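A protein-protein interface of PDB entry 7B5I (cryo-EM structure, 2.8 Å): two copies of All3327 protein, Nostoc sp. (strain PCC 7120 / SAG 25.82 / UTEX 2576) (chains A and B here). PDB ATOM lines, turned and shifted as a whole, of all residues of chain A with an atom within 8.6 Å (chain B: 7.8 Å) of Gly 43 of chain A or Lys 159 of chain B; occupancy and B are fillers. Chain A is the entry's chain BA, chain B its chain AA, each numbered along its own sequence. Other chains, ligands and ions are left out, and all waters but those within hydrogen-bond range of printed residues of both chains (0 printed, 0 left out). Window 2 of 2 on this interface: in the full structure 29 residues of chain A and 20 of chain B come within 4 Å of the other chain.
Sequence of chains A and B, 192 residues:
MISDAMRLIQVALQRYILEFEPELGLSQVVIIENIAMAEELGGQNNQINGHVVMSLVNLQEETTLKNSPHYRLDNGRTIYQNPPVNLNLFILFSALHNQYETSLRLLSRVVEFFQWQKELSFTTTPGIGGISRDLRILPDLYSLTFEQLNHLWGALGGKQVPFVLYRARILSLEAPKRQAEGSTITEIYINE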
ATOM      1  N   ASN A  34     -10.280  16.692  10.585  1.00  0.00           N
ATOM      2  CA  ASN A  34      -9.832  17.087  11.913  1.00  0.00           C
ATOM      3  C   ASN A  34     -10.652  18.280  12.385  1.00  0.00           C
ATOM      4  O   ASN A  34     -10.773  19.277  11.669  1.00  0.00           O
ATOM      5  CB  ASN A  34      -8.347  17.442  11.901  1.00  0.00           C
ATOM      6  CG  ASN A  34      -7.761  17.550  13.293  1.00  0.00           C
ATOM      7  OD1 ASN A  34      -8.477  17.497  14.289  1.00  0.00           O
ATOM      8  ND2 ASN A  34      -6.448  17.707  13.367  1.00  0.00           N
ATOM      9  N   ILE A  35     -11.213  18.175  13.591  1.00  0.00           N
ATOM     10  CA  ILE A  35     -12.110  19.217  14.075  1.00  0.00           C
ATOM     11  C   ILE A  35     -11.331  20.460  14.486  1.00  0.00           C
ATOM     12  O   ILE A  35     -11.779  21.589  14.258  1.00  0.00           O
ATOM     13  CB  ILE A  35     -12.982  18.685  15.226  1.00  0.00           C
ATOM     14  CG1 ILE A  35     -13.954  19.763  15.695  1.00  0.00           C
ATOM     15  CG2 ILE A  35     -12.133  18.210  16.382  1.00  0.00           C
ATOM     16  CD1 ILE A  35     -14.886  20.250  14.617  1.00  0.00           C
ATOM     17  N   ALA A  36     -10.152  20.279  15.082  1.00  0.00           N
ATOM     18  CA  ALA A  36      -9.393  21.407  15.604  1.00  0.00           C
ATOM     19  C   ALA A  36      -8.962  22.381  14.519  1.00  0.00           C
ATOM     20  O   ALA A  36      -8.586  23.512  14.840  1.00  0.00           O
ATOM     21  CB  ALA A  36      -8.165  20.903  16.361  1.00  0.00           C
ATOM     22  N   MET A  37      -9.013  21.979  13.256  1.00  0.00           N
ATOM     23  CA  MET A  37      -8.619  22.838  12.151  1.00  0.00           C
ATOM     24  C   MET A  37      -9.717  23.796  11.721  1.00  0.00           C
ATOM     25  O   MET A  37      -9.511  24.558  10.773  1.00  0.00           O
ATOM     26  CB  MET A  37      -8.196  21.981  10.958  1.00  0.00           C
ATOM     27  CG  MET A  37      -7.037  21.046  11.242  1.00  0.00           C
ATOM     28  SD  MET A  37      -5.501  21.913  11.594  1.00  0.00           S
ATOM     29  CE  MET A  37      -5.342  21.613  13.350  1.00  0.00           C
ATOM     30  N   ALA A  38     -10.869  23.777  12.382  1.00  0.00           N
ATOM     31  CA  ALA A  38     -11.990  24.598  11.954  1.00  0.00           C
ATOM     32  C   ALA A  38     -11.716  26.073  12.210  1.00  0.00           C
ATOM     33  O   ALA A  38     -11.125  26.447  13.227  1.00  0.00           O
ATOM     34  CB  ALA A  38     -13.266  24.173  12.675  1.00  0.00           C
ATOM     35  N   GLU A  39     -12.162  26.913  11.278  1.00  0.00           N
ATOM     36  CA  GLU A  39     -11.947  28.349  11.397  1.00  0.00           C
ATOM     37  C   GLU A  39     -12.676  28.926  12.600  1.00  0.00           C
ATOM     38  O   GLU A  39     -12.149  29.803  13.294  1.00  0.00           O
ATOM     39  CB  GLU A  39     -12.402  29.043  10.119  1.00  0.00           C
ATOM     40  CG  GLU A  39     -12.306  30.542  10.156  1.00  0.00           C
ATOM     41  CD  GLU A  39     -12.785  31.168   8.868  1.00  0.00           C
ATOM     42  OE1 GLU A  39     -13.830  30.727   8.347  1.00  0.00           O
ATOM     43  OE2 GLU A  39     -12.115  32.095   8.372  1.00  0.00           O
ATOM     44  N   GLU A  40     -13.894  28.452  12.861  1.00  0.00           N
ATOM     45  CA  GLU A  40     -14.698  29.008  13.942  1.00  0.00           C
ATOM     46  C   GLU A  40     -14.073  28.776  15.308  1.00  0.00           C
ATOM     47  O   GLU A  40     -14.337  29.548  16.234  1.00  0.00           O
ATOM     48  CB  GLU A  40     -16.106  28.412  13.909  1.00  0.00           C
ATOM     49  CG  GLU A  40     -16.938  28.853  12.718  1.00  0.00           C
ATOM     50  CD  GLU A  40     -16.601  28.087  11.457  1.00  0.00           C
ATOM     51  OE1 GLU A  40     -15.843  27.102  11.546  1.00  0.00           O
ATOM     52  OE2 GLU A  40     -17.086  28.473  10.374  1.00  0.00           O
ATOM     53  N   LEU A  41     -13.251  27.744  15.455  1.00  0.00           N
ATOM     54  CA  LEU A  41     -12.595  27.451  16.718  1.00  0.00           C
ATOM     55  C   LEU A  41     -11.182  28.010  16.784  1.00  0.00           C
ATOM     56  O   LEU A  41     -10.419  27.636  17.679  1.00  0.00           O
ATOM     57  CB  LEU A  41     -12.570  25.944  16.962  1.00  0.00           C
ATOM     58  CG  LEU A  41     -13.905  25.205  16.873  1.00  0.00           C
ATOM     59  CD1 LEU A  41     -13.691  23.729  17.125  1.00  0.00           C
ATOM     60  CD2 LEU A  41     -14.913  25.772  17.848  1.00  0.00           C
ATOM     61  N   GLY A  42     -10.814  28.889  15.856  1.00  0.00           N
ATOM     62  CA  GLY A  42      -9.501  29.495  15.840  1.00  0.00           C
ATOM     63  C   GLY A  42      -8.524  28.901  14.851  1.00  0.00           C
ATOM     64  O   GLY A  42      -7.370  29.341  14.814  1.00  0.00           O
ATOM     65  N   GLY A  43      -8.944  27.935  14.043  1.00  0.00           N
ATOM     66  CA  GLY A  43      -8.080  27.311  13.066  1.00  0.00           C
ATOM     67  C   GLY A  43      -8.026  28.085  11.767  1.00  0.00           C
ATOM     68  O   GLY A  43      -8.309  29.284  11.712  1.00  0.00           O
ATOM     69  N   GLN A  44      -7.665  27.374  10.699  1.00  0.00           N
ATOM     70  CA  GLN A  44      -7.444  27.987   9.399  1.00  0.00           C
ATOM     71  C   GLN A  44      -8.359  27.470   8.303  1.00  0.00           C
ATOM     72  O   GLN A  44      -8.475  28.131   7.266  1.00  0.00           O
ATOM     73  CB  GLN A  44      -5.991  27.774   8.945  1.00  0.00           C
ATOM     74  CG  GLN A  44      -4.940  28.142   9.978  1.00  0.00           C
ATOM     75  CD  GLN A  44      -4.921  29.620  10.299  1.00  0.00           C
ATOM     76  OE1 GLN A  44      -4.891  30.459   9.402  1.00  0.00           O
ATOM     77  NE2 GLN A  44      -4.930  29.946  11.585  1.00  0.00           N
ATOM     78  N   ASN A  45      -8.995  26.317   8.487  1.00  0.00           N
ATOM     79  CA  ASN A  45      -9.820  25.706   7.453  1.00  0.00           C
ATOM     80  C   ASN A  45     -11.221  26.299   7.494  1.00  0.00           C
ATOM     81  O   ASN A  45     -11.852  26.339   8.554  1.00  0.00           O
ATOM     82  CB  ASN A  45      -9.872  24.191   7.648  1.00  0.00           C
ATOM     83  CG  ASN A  45     -10.416  23.461   6.441  1.00  0.00           C
ATOM     84  OD1 ASN A  45     -11.268  23.974   5.717  1.00  0.00           O
ATOM     85  ND2 ASN A  45      -9.927  22.250   6.221  1.00  0.00           N
ATOM     86  N   ASN A  46     -11.707  26.757   6.340  1.00  0.00           N
ATOM     87  CA  ASN A  46     -13.018  27.385   6.246  1.00  0.00           C
ATOM     88  C   ASN A  46     -14.053  26.509   5.552  1.00  0.00           C
ATOM     89  O   ASN A  46     -15.116  27.009   5.176  1.00  0.00           O
ATOM     90  CB  ASN A  46     -12.912  28.729   5.524  1.00  0.00           C
ATOM     91  CG  ASN A  46     -12.332  28.600   4.138  1.00  0.00           C
ATOM     92  OD1 ASN A  46     -11.607  27.651   3.845  1.00  0.00           O
ATOM     93  ND2 ASN A  46     -12.654  29.549   3.269  1.00  0.00           N
ATOM     94  N   ILE A  48     -15.076  23.394   6.950  1.00  0.00           N
ATOM     95  CA  ILE A  48     -15.718  22.546   7.949  1.00  0.00           C
ATOM     96  C   ILE A  48     -16.787  23.401   8.617  1.00  0.00           C
ATOM     97  O   ILE A  48     -16.537  24.088   9.608  1.00  0.00           O
ATOM     98  CB  ILE A  48     -14.714  21.994   8.954  1.00  0.00           C
ATOM     99  CG1 ILE A  48     -13.490  21.435   8.234  1.00  0.00           C
ATOM    100  CG2 ILE A  48     -15.358  20.927   9.808  1.00  0.00           C
ATOM    101  CD1 ILE A  48     -12.319  21.212   9.144  1.00  0.00           C
ATOM    102  N   LEU A 152      -9.693  16.452  27.337  1.00  0.00           N
ATOM    103  CA  LEU A 152      -9.962  16.250  25.919  1.00  0.00           C
ATOM    104  C   LEU A 152      -9.907  17.564  25.145  1.00  0.00           C
ATOM    105  O   LEU A 152      -9.121  17.723  24.201  1.00  0.00           O
ATOM    106  CB  LEU A 152     -11.327  15.586  25.755  1.00  0.00           C
ATOM    107  CG  LEU A 152     -11.725  15.220  24.330  1.00  0.00           C
ATOM    108  CD1 LEU A 152     -10.900  14.044  23.844  1.00  0.00           C
ATOM    109  CD2 LEU A 152     -13.206  14.913  24.250  1.00  0.00           C
ATOM    110  N   TRP A 153     -10.731  18.526  25.538  1.00  0.00           N
ATOM    111  CA  TRP A 153     -10.832  19.743  24.751  1.00  0.00           C
ATOM    112  C   TRP A 153      -9.643  20.670  24.950  1.00  0.00           C
ATOM    113  O   TRP A 153      -9.423  21.550  24.116  1.00  0.00           O
ATOM    114  CB  TRP A 153     -12.144  20.454  25.063  1.00  0.00           C
ATOM    115  CG  TRP A 153     -13.305  19.743  24.453  1.00  0.00           C
ATOM    116  CD1 TRP A 153     -14.223  18.972  25.096  1.00  0.00           C
ATOM    117  CD2 TRP A 153     -13.651  19.707  23.066  1.00  0.00           C
ATOM    118  NE1 TRP A 153     -15.130  18.469  24.199  1.00  0.00           N
ATOM    119  CE2 TRP A 153     -14.800  18.906  22.945  1.00  0.00           C
ATOM    120  CE3 TRP A 153     -13.104  20.279  21.917  1.00  0.00           C
ATOM    121  CZ2 TRP A 153     -15.413  18.664  21.719  1.00  0.00           C
ATOM    122  CZ3 TRP A 153     -13.715  20.041  20.703  1.00  0.00           C
ATOM    123  CH2 TRP A 153     -14.858  19.240  20.613  1.00  0.00           C
ATOM    124  N   GLY A 154      -8.860  20.484  26.013  1.00  0.00           N
ATOM    125  CA  GLY A 154      -7.577  21.156  26.089  1.00  0.00           C
ATOM    126  C   GLY A 154      -6.592  20.595  25.089  1.00  0.00           C
ATOM    127  O   GLY A 154      -5.796  21.334  24.507  1.00  0.00           O
ATOM    128  N   ALA A 155      -6.634  19.281  24.869  1.00  0.00           N
ATOM    129  CA  ALA A 155      -5.840  18.707  23.790  1.00  0.00           C
ATOM    130  C   ALA A 155      -6.377  19.069  22.413  1.00  0.00           C
ATOM    131  O   ALA A 155      -5.654  18.914  21.425  1.00  0.00           O
ATOM    132  CB  ALA A 155      -5.766  17.188  23.924  1.00  0.00           C
ATOM    133  N   LEU A 156      -7.627  19.521  22.314  1.00  0.00           N
ATOM    134  CA  LEU A 156      -8.221  19.821  21.014  1.00  0.00           C
ATOM    135  C   LEU A 156      -8.385  21.306  20.712  1.00  0.00           C
ATOM    136  O   LEU A 156      -8.945  21.641  19.664  1.00  0.00           O
ATOM    137  CB  LEU A 156      -9.577  19.127  20.876  1.00  0.00           C
ATOM    138  CG  LEU A 156      -9.505  17.621  20.653  1.00  0.00           C
ATOM    139  CD1 LEU A 156     -10.885  17.014  20.676  1.00  0.00           C
ATOM    140  CD2 LEU A 156      -8.815  17.340  19.334  1.00  0.00           C
ATOM    141  N   GLY A 157      -7.922  22.203  21.575  1.00  0.00           N
ATOM    142  CA  GLY A 157      -7.952  23.630  21.309  1.00  0.00           C
ATOM    143  C   GLY A 157      -8.636  24.471  22.369  1.00  0.00           C
ATOM    144  O   GLY A 157      -8.336  25.669  22.476  1.00  0.00           O
ATOM    145  N   GLY A 158      -9.547  23.904  23.148  1.00  0.00           N
ATOM    146  CA  GLY A 158     -10.139  24.613  24.260  1.00  0.00           C
ATOM    147  C   GLY A 158     -11.524  25.187  24.057  1.00  0.00           C
ATOM    148  O   GLY A 158     -11.885  26.122  24.776  1.00  0.00           O
ATOM    149  N   ILE B  35       7.639  19.565  15.102  1.00  0.00           N
ATOM    150  CA  ILE B  35       6.244  19.633  14.684  1.00  0.00           C
ATOM    151  C   ILE B  35       5.603  20.939  15.135  1.00  0.00           C
ATOM    152  O   ILE B  35       4.798  21.531  14.409  1.00  0.00           O
ATOM    153  CB  ILE B  35       5.467  18.409  15.199  1.00  0.00           C
ATOM    154  CG1 ILE B  35       4.020  18.461  14.716  1.00  0.00           C
ATOM    155  CG2 ILE B  35       5.510  18.328  16.707  1.00  0.00           C
ATOM    156  CD1 ILE B  35       3.882  18.479  13.217  1.00  0.00           C
ATOM    157  N   GLU B  40       0.213  25.519  10.335  1.00  0.00           N
ATOM    158  CA  GLU B  40      -1.179  25.149  10.556  1.00  0.00           C
ATOM    159  C   GLU B  40      -1.526  25.051  12.032  1.00  0.00           C
ATOM    160  O   GLU B  40      -2.693  25.221  12.394  1.00  0.00           O
ATOM    161  CB  GLU B  40      -1.487  23.822   9.863  1.00  0.00           C
ATOM    162  CG  GLU B  40      -1.480  23.898   8.346  1.00  0.00           C
ATOM    163  CD  GLU B  40      -0.081  23.859   7.768  1.00  0.00           C
ATOM    164  OE1 GLU B  40       0.870  23.605   8.532  1.00  0.00           O
ATOM    165  OE2 GLU B  40       0.070  24.092   6.552  1.00  0.00           O
ATOM    166  N   LEU B  41      -0.546  24.790  12.891  1.00  0.00           N
ATOM    167  CA  LEU B  41      -0.779  24.690  14.322  1.00  0.00           C
ATOM    168  C   LEU B  41      -0.465  25.987  15.054  1.00  0.00           C
ATOM    169  O   LEU B  41      -0.375  25.987  16.285  1.00  0.00           O
ATOM    170  CB  LEU B  41       0.046  23.549  14.913  1.00  0.00           C
ATOM    171  CG  LEU B  41      -0.100  22.176  14.255  1.00  0.00           C
ATOM    172  CD1 LEU B  41       0.794  21.176  14.953  1.00  0.00           C
ATOM    173  CD2 LEU B  41      -1.539  21.710  14.273  1.00  0.00           C
ATOM    174  N   GLY B  42      -0.291  27.088  14.327  1.00  0.00           N
ATOM    175  CA  GLY B  42      -0.009  28.373  14.925  1.00  0.00           C
ATOM    176  C   GLY B  42       1.440  28.805  14.885  1.00  0.00           C
ATOM    177  O   GLY B  42       1.760  29.873  15.417  1.00  0.00           O
ATOM    178  N   LEU B 152       1.382  15.964  27.024  1.00  0.00           N
ATOM    179  CA  LEU B 152       2.212  15.987  25.827  1.00  0.00           C
ATOM    180  C   LEU B 152       1.865  17.167  24.924  1.00  0.00           C
ATOM    181  O   LEU B 152       2.713  18.014  24.615  1.00  0.00           O
ATOM    182  CB  LEU B 152       2.048  14.668  25.075  1.00  0.00           C
ATOM    183  CG  LEU B 152       2.922  14.490  23.839  1.00  0.00           C
ATOM    184  CD1 LEU B 152       4.367  14.278  24.247  1.00  0.00           C
ATOM    185  CD2 LEU B 152       2.423  13.337  22.992  1.00  0.00           C
ATOM    186  N   TRP B 153       0.610  17.246  24.499  1.00  0.00           N
ATOM    187  CA  TRP B 153       0.252  18.260  23.522  1.00  0.00           C
ATOM    188  C   TRP B 153       0.141  19.648  24.130  1.00  0.00           C
ATOM    189  O   TRP B 153       0.185  20.633  23.390  1.00  0.00           O
ATOM    190  CB  TRP B 153      -1.039  17.862  22.814  1.00  0.00           C
ATOM    191  CG  TRP B 153      -0.808  16.748  21.849  1.00  0.00           C
ATOM    192  CD1 TRP B 153      -1.159  15.442  22.008  1.00  0.00           C
ATOM    193  CD2 TRP B 153      -0.141  16.835  20.588  1.00  0.00           C
ATOM    194  NE1 TRP B 153      -0.764  14.711  20.917  1.00  0.00           N
ATOM    195  CE2 TRP B 153      -0.135  15.544  20.030  1.00  0.00           C
ATOM    196  CE3 TRP B 153       0.448  17.880  19.874  1.00  0.00           C
ATOM    197  CZ2 TRP B 153       0.434  15.271  18.791  1.00  0.00           C
ATOM    198  CZ3 TRP B 153       1.010  17.608  18.644  1.00  0.00           C
ATOM    199  CH2 TRP B 153       0.999  16.313  18.114  1.00  0.00           C
ATOM    200  N   GLY B 154       0.024  19.758  25.454  1.00  0.00           N
ATOM    201  CA  GLY B 154       0.194  21.051  26.088  1.00  0.00           C
ATOM    202  C   GLY B 154       1.633  21.513  26.035  1.00  0.00           C
ATOM    203  O   GLY B 154       1.906  22.703  25.862  1.00  0.00           O
ATOM    204  N   LEU B 156       3.433  20.737  23.570  1.00  0.00           N
ATOM    205  CA  LEU B 156       3.713  20.890  22.145  1.00  0.00           C
ATOM    206  C   LEU B 156       2.868  21.939  21.434  1.00  0.00           C
ATOM    207  O   LEU B 156       2.992  22.079  20.215  1.00  0.00           O
ATOM    208  CB  LEU B 156       3.557  19.548  21.426  1.00  0.00           C
ATOM    209  CG  LEU B 156       4.679  18.550  21.683  1.00  0.00           C
ATOM    210  CD1 LEU B 156       4.360  17.218  21.052  1.00  0.00           C
ATOM    211  CD2 LEU B 156       5.979  19.105  21.141  1.00  0.00           C
ATOM    212  N   GLY B 157       2.021  22.682  22.139  1.00  0.00           N
ATOM    213  CA  GLY B 157       1.258  23.769  21.550  1.00  0.00           C
ATOM    214  C   GLY B 157      -0.242  23.688  21.751  1.00  0.00           C
ATOM    215  O   GLY B 157      -0.914  24.728  21.701  1.00  0.00           O
ATOM    216  N   GLY B 158      -0.798  22.504  21.967  1.00  0.00           N
ATOM    217  CA  GLY B 158      -2.200  22.374  22.296  1.00  0.00           C
ATOM    218  C   GLY B 158      -3.136  21.955  21.184  1.00  0.00           C
ATOM    219  O   GLY B 158      -4.334  22.231  21.286  1.00  0.00           O
ATOM    220  N   LYS B 159      -2.642  21.305  20.132  1.00  0.00           N
ATOM    221  CA  LYS B 159      -3.497  20.801  19.063  1.00  0.00           C
ATOM    222  C   LYS B 159      -2.950  19.490  18.524  1.00  0.00           C
ATOM    223  O   LYS B 159      -1.755  19.381  18.240  1.00  0.00           O
ATOM    224  CB  LYS B 159      -3.624  21.812  17.923  1.00  0.00           C
ATOM    225  CG  LYS B 159      -4.575  22.943  18.212  1.00  0.00           C
ATOM    226  CD  LYS B 159      -4.840  23.761  16.973  1.00  0.00           C
ATOM    227  CE  LYS B 159      -5.914  24.796  17.227  1.00  0.00           C
ATOM    228  NZ  LYS B 159      -6.212  25.588  16.007  1.00  0.00           N
ATOM    229  N   GLN B 160      -3.831  18.510  18.362  1.00  0.00           N
ATOM    230  CA  GLN B 160      -3.464  17.168  17.939  1.00  0.00           C
ATOM    231  C   GLN B 160      -3.446  17.024  16.423  1.00  0.00           C
ATOM    232  O   GLN B 160      -4.121  17.749  15.690  1.00  0.00           O
ATOM    233  CB  GLN B 160      -4.442  16.138  18.489  1.00  0.00           C
ATOM    234  CG  GLN B 160      -4.268  15.744  19.913  1.00  0.00           C
ATOM    235  CD  GLN B 160      -5.209  14.621  20.267  1.00  0.00           C
ATOM    236  OE1 GLN B 160      -5.491  13.760  19.439  1.00  0.00           O
ATOM    237  NE2 GLN B 160      -5.711  14.627  21.492  1.00  0.00           N
ATOM    238  N   VAL B 161      -2.671  16.045  15.967  1.00  0.00           N
ATOM    239  CA  VAL B 161      -2.755  15.494  14.617  1.00  0.00           C
ATOM    240  C   VAL B 161      -2.685  13.981  14.784  1.00  0.00           C
ATOM    241  O   VAL B 161      -2.386  13.511  15.889  1.00  0.00           O
ATOM    242  CB  VAL B 161      -1.634  16.023  13.710  1.00  0.00           C
ATOM    243  CG1 VAL B 161      -1.832  17.493  13.414  1.00  0.00           C
ATOM    244  CG2 VAL B 161      -0.286  15.775  14.344  1.00  0.00           C
ATOM    245  N   PRO B 162      -2.967  13.181  13.758  1.00  0.00           N
ATOM    246  CA  PRO B 162      -2.740  11.734  13.881  1.00  0.00           C
ATOM    247  C   PRO B 162      -1.274  11.440  14.165  1.00  0.00           C
ATOM    248  O   PRO B 162      -0.385  11.882  13.437  1.00  0.00           O
ATOM    249  CB  PRO B 162      -3.174  11.194  12.515  1.00  0.00           C
ATOM    250  CG  PRO B 162      -4.137  12.193  12.007  1.00  0.00           C
ATOM    251  CD  PRO B 162      -3.654  13.521  12.501  1.00  0.00           C
ATOM    252  N   PHE B 163      -1.024  10.675  15.224  1.00  0.00           N
ATOM    253  CA  PHE B 163       0.336  10.516  15.721  1.00  0.00           C
ATOM    254  C   PHE B 163       0.512   9.142  16.345  1.00  0.00           C
ATOM    255  O   PHE B 163      -0.446   8.395  16.547  1.00  0.00           O
ATOM    256  CB  PHE B 163       0.677  11.592  16.754  1.00  0.00           C
ATOM    257  CG  PHE B 163       0.006  11.381  18.076  1.00  0.00           C
ATOM    258  CD1 PHE B 163      -1.256  11.883  18.307  1.00  0.00           C
ATOM    259  CD2 PHE B 163       0.632  10.671  19.083  1.00  0.00           C
ATOM    260  CE1 PHE B 163      -1.879  11.684  19.510  1.00  0.00           C
ATOM    261  CE2 PHE B 163       0.014  10.467  20.286  1.00  0.00           C
ATOM    262  CZ  PHE B 163      -1.244  10.975  20.500  1.00  0.00           C
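Among the printed residues, pairs that only touch across the chains: Ala 155 of chain A with Gln 160 of chain B, Ala 155 of chain A with Gly 158 of chain B, Gly 157 of chain A with Gly 158 of chain B, Gly 154 of chain A with Gly 158 of chain B, Ala 155 of chain A with Lys 159 of chain B, Gly 43 of chain A with Lys 159 of chain B and Met 37 of chain A with Leu 41 of chain B.
The side-chain amino group of Lys 159 of chain B sits at hydrogen-bond distance from the backbone carbonyl oxygen of Ala 36 of chain A (3.4 Å). ND2 of Asn 34 of chain A sits at hydrogen-bond distance from O of Gln 160 of chain B (3.3 Å).
Of the 15 printed residues of chain B, 4 touch a printed residue of chain A. Hydrophobic or aromatic side chains of chain B within 4 Å of the printed part of chain A: Leu 41. Hydrophobic or aromatic side chains of chain A within 4 Å of the printed part of chain B: Met 37 and Ala 155. Among the printed residues, 9 pairs touch across the chains. Among the printed residues, no Asp or Glu carboxylate lies within 4 Å of a Lys or Arg side-chain nitrogen of the other chain.
Gly 154 of chain A touches Gly 158 of chain B, but with the chains exchanged Gly 158 of chain A does not touch Gly 154 of chain B (10.6 Å). Gly 157 of chain A touches Gly 158 of chain B, but with the chains exchanged Gly 158 of chain A does not touch Gly 157 of chain B (8.8 Å). Positions printed for both chains: 35, 40, 41, 42, 152, 153, 154, 156, 157 and 158.
The backbone NH (N) of Gly 158 of chain B sits at hydrogen-bond distance from the backbone carbonyl oxygen (O) of Trp 153 of chain B. OD1 of Asn 34 of chain A lies within hydrogen-bond range of N of Ala 36 of chain A, 3.3 Å away. O of Met 37 of chain A sits at hydrogen-bond distance from N of Gln 44 of chain A (3.4 Å). The backbone NH (N) of Asn 45 of chain A sits at hydrogen-bond distance from the backbone carbonyl oxygen (O) of Met 37 of chain A (2.9 Å). The backbone carbonyl oxygen of Ala 38 of chain A is in hydrogen-bond range of the backbone NH of Gly 43 of chain A.
Ala 38 of chain A touches none of the printed residues of chain B. No residue of chain B comes within 4 Å of Gly 42 of chain A. Of chain B, only Lys 159 comes within 4 Å of Gly 43 of chain A. Printed residues of chain B within 4 Å of Ala 155 of chain A: Gly 158 (3.6 Å), Lys 159 (3.7 Å) and Gln 160 (3.5 Å). Of the printed residues of chain B, Gly 157 of chain A touches Gly 158 (3.6 Å). Gly 42 of chain B touches none of the printed residues of chain A. Of chain A, only Gly 154, Ala 155 and Gly 157 come within 4 Å of Gly 158 of chain B. Lys 159 of chain B touches just these residues of chain A: Ala 36, Gly 43 and Ala 155. Of the printed residues of chain A, Gln 160 of chain B touches Asn 34 (3.3 Å) and Ala 155 (3.5 Å). The nearest printed residue of chain B that does not touch Ala 36 of chain A is Gln 160 of chain B (5.2 Å).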
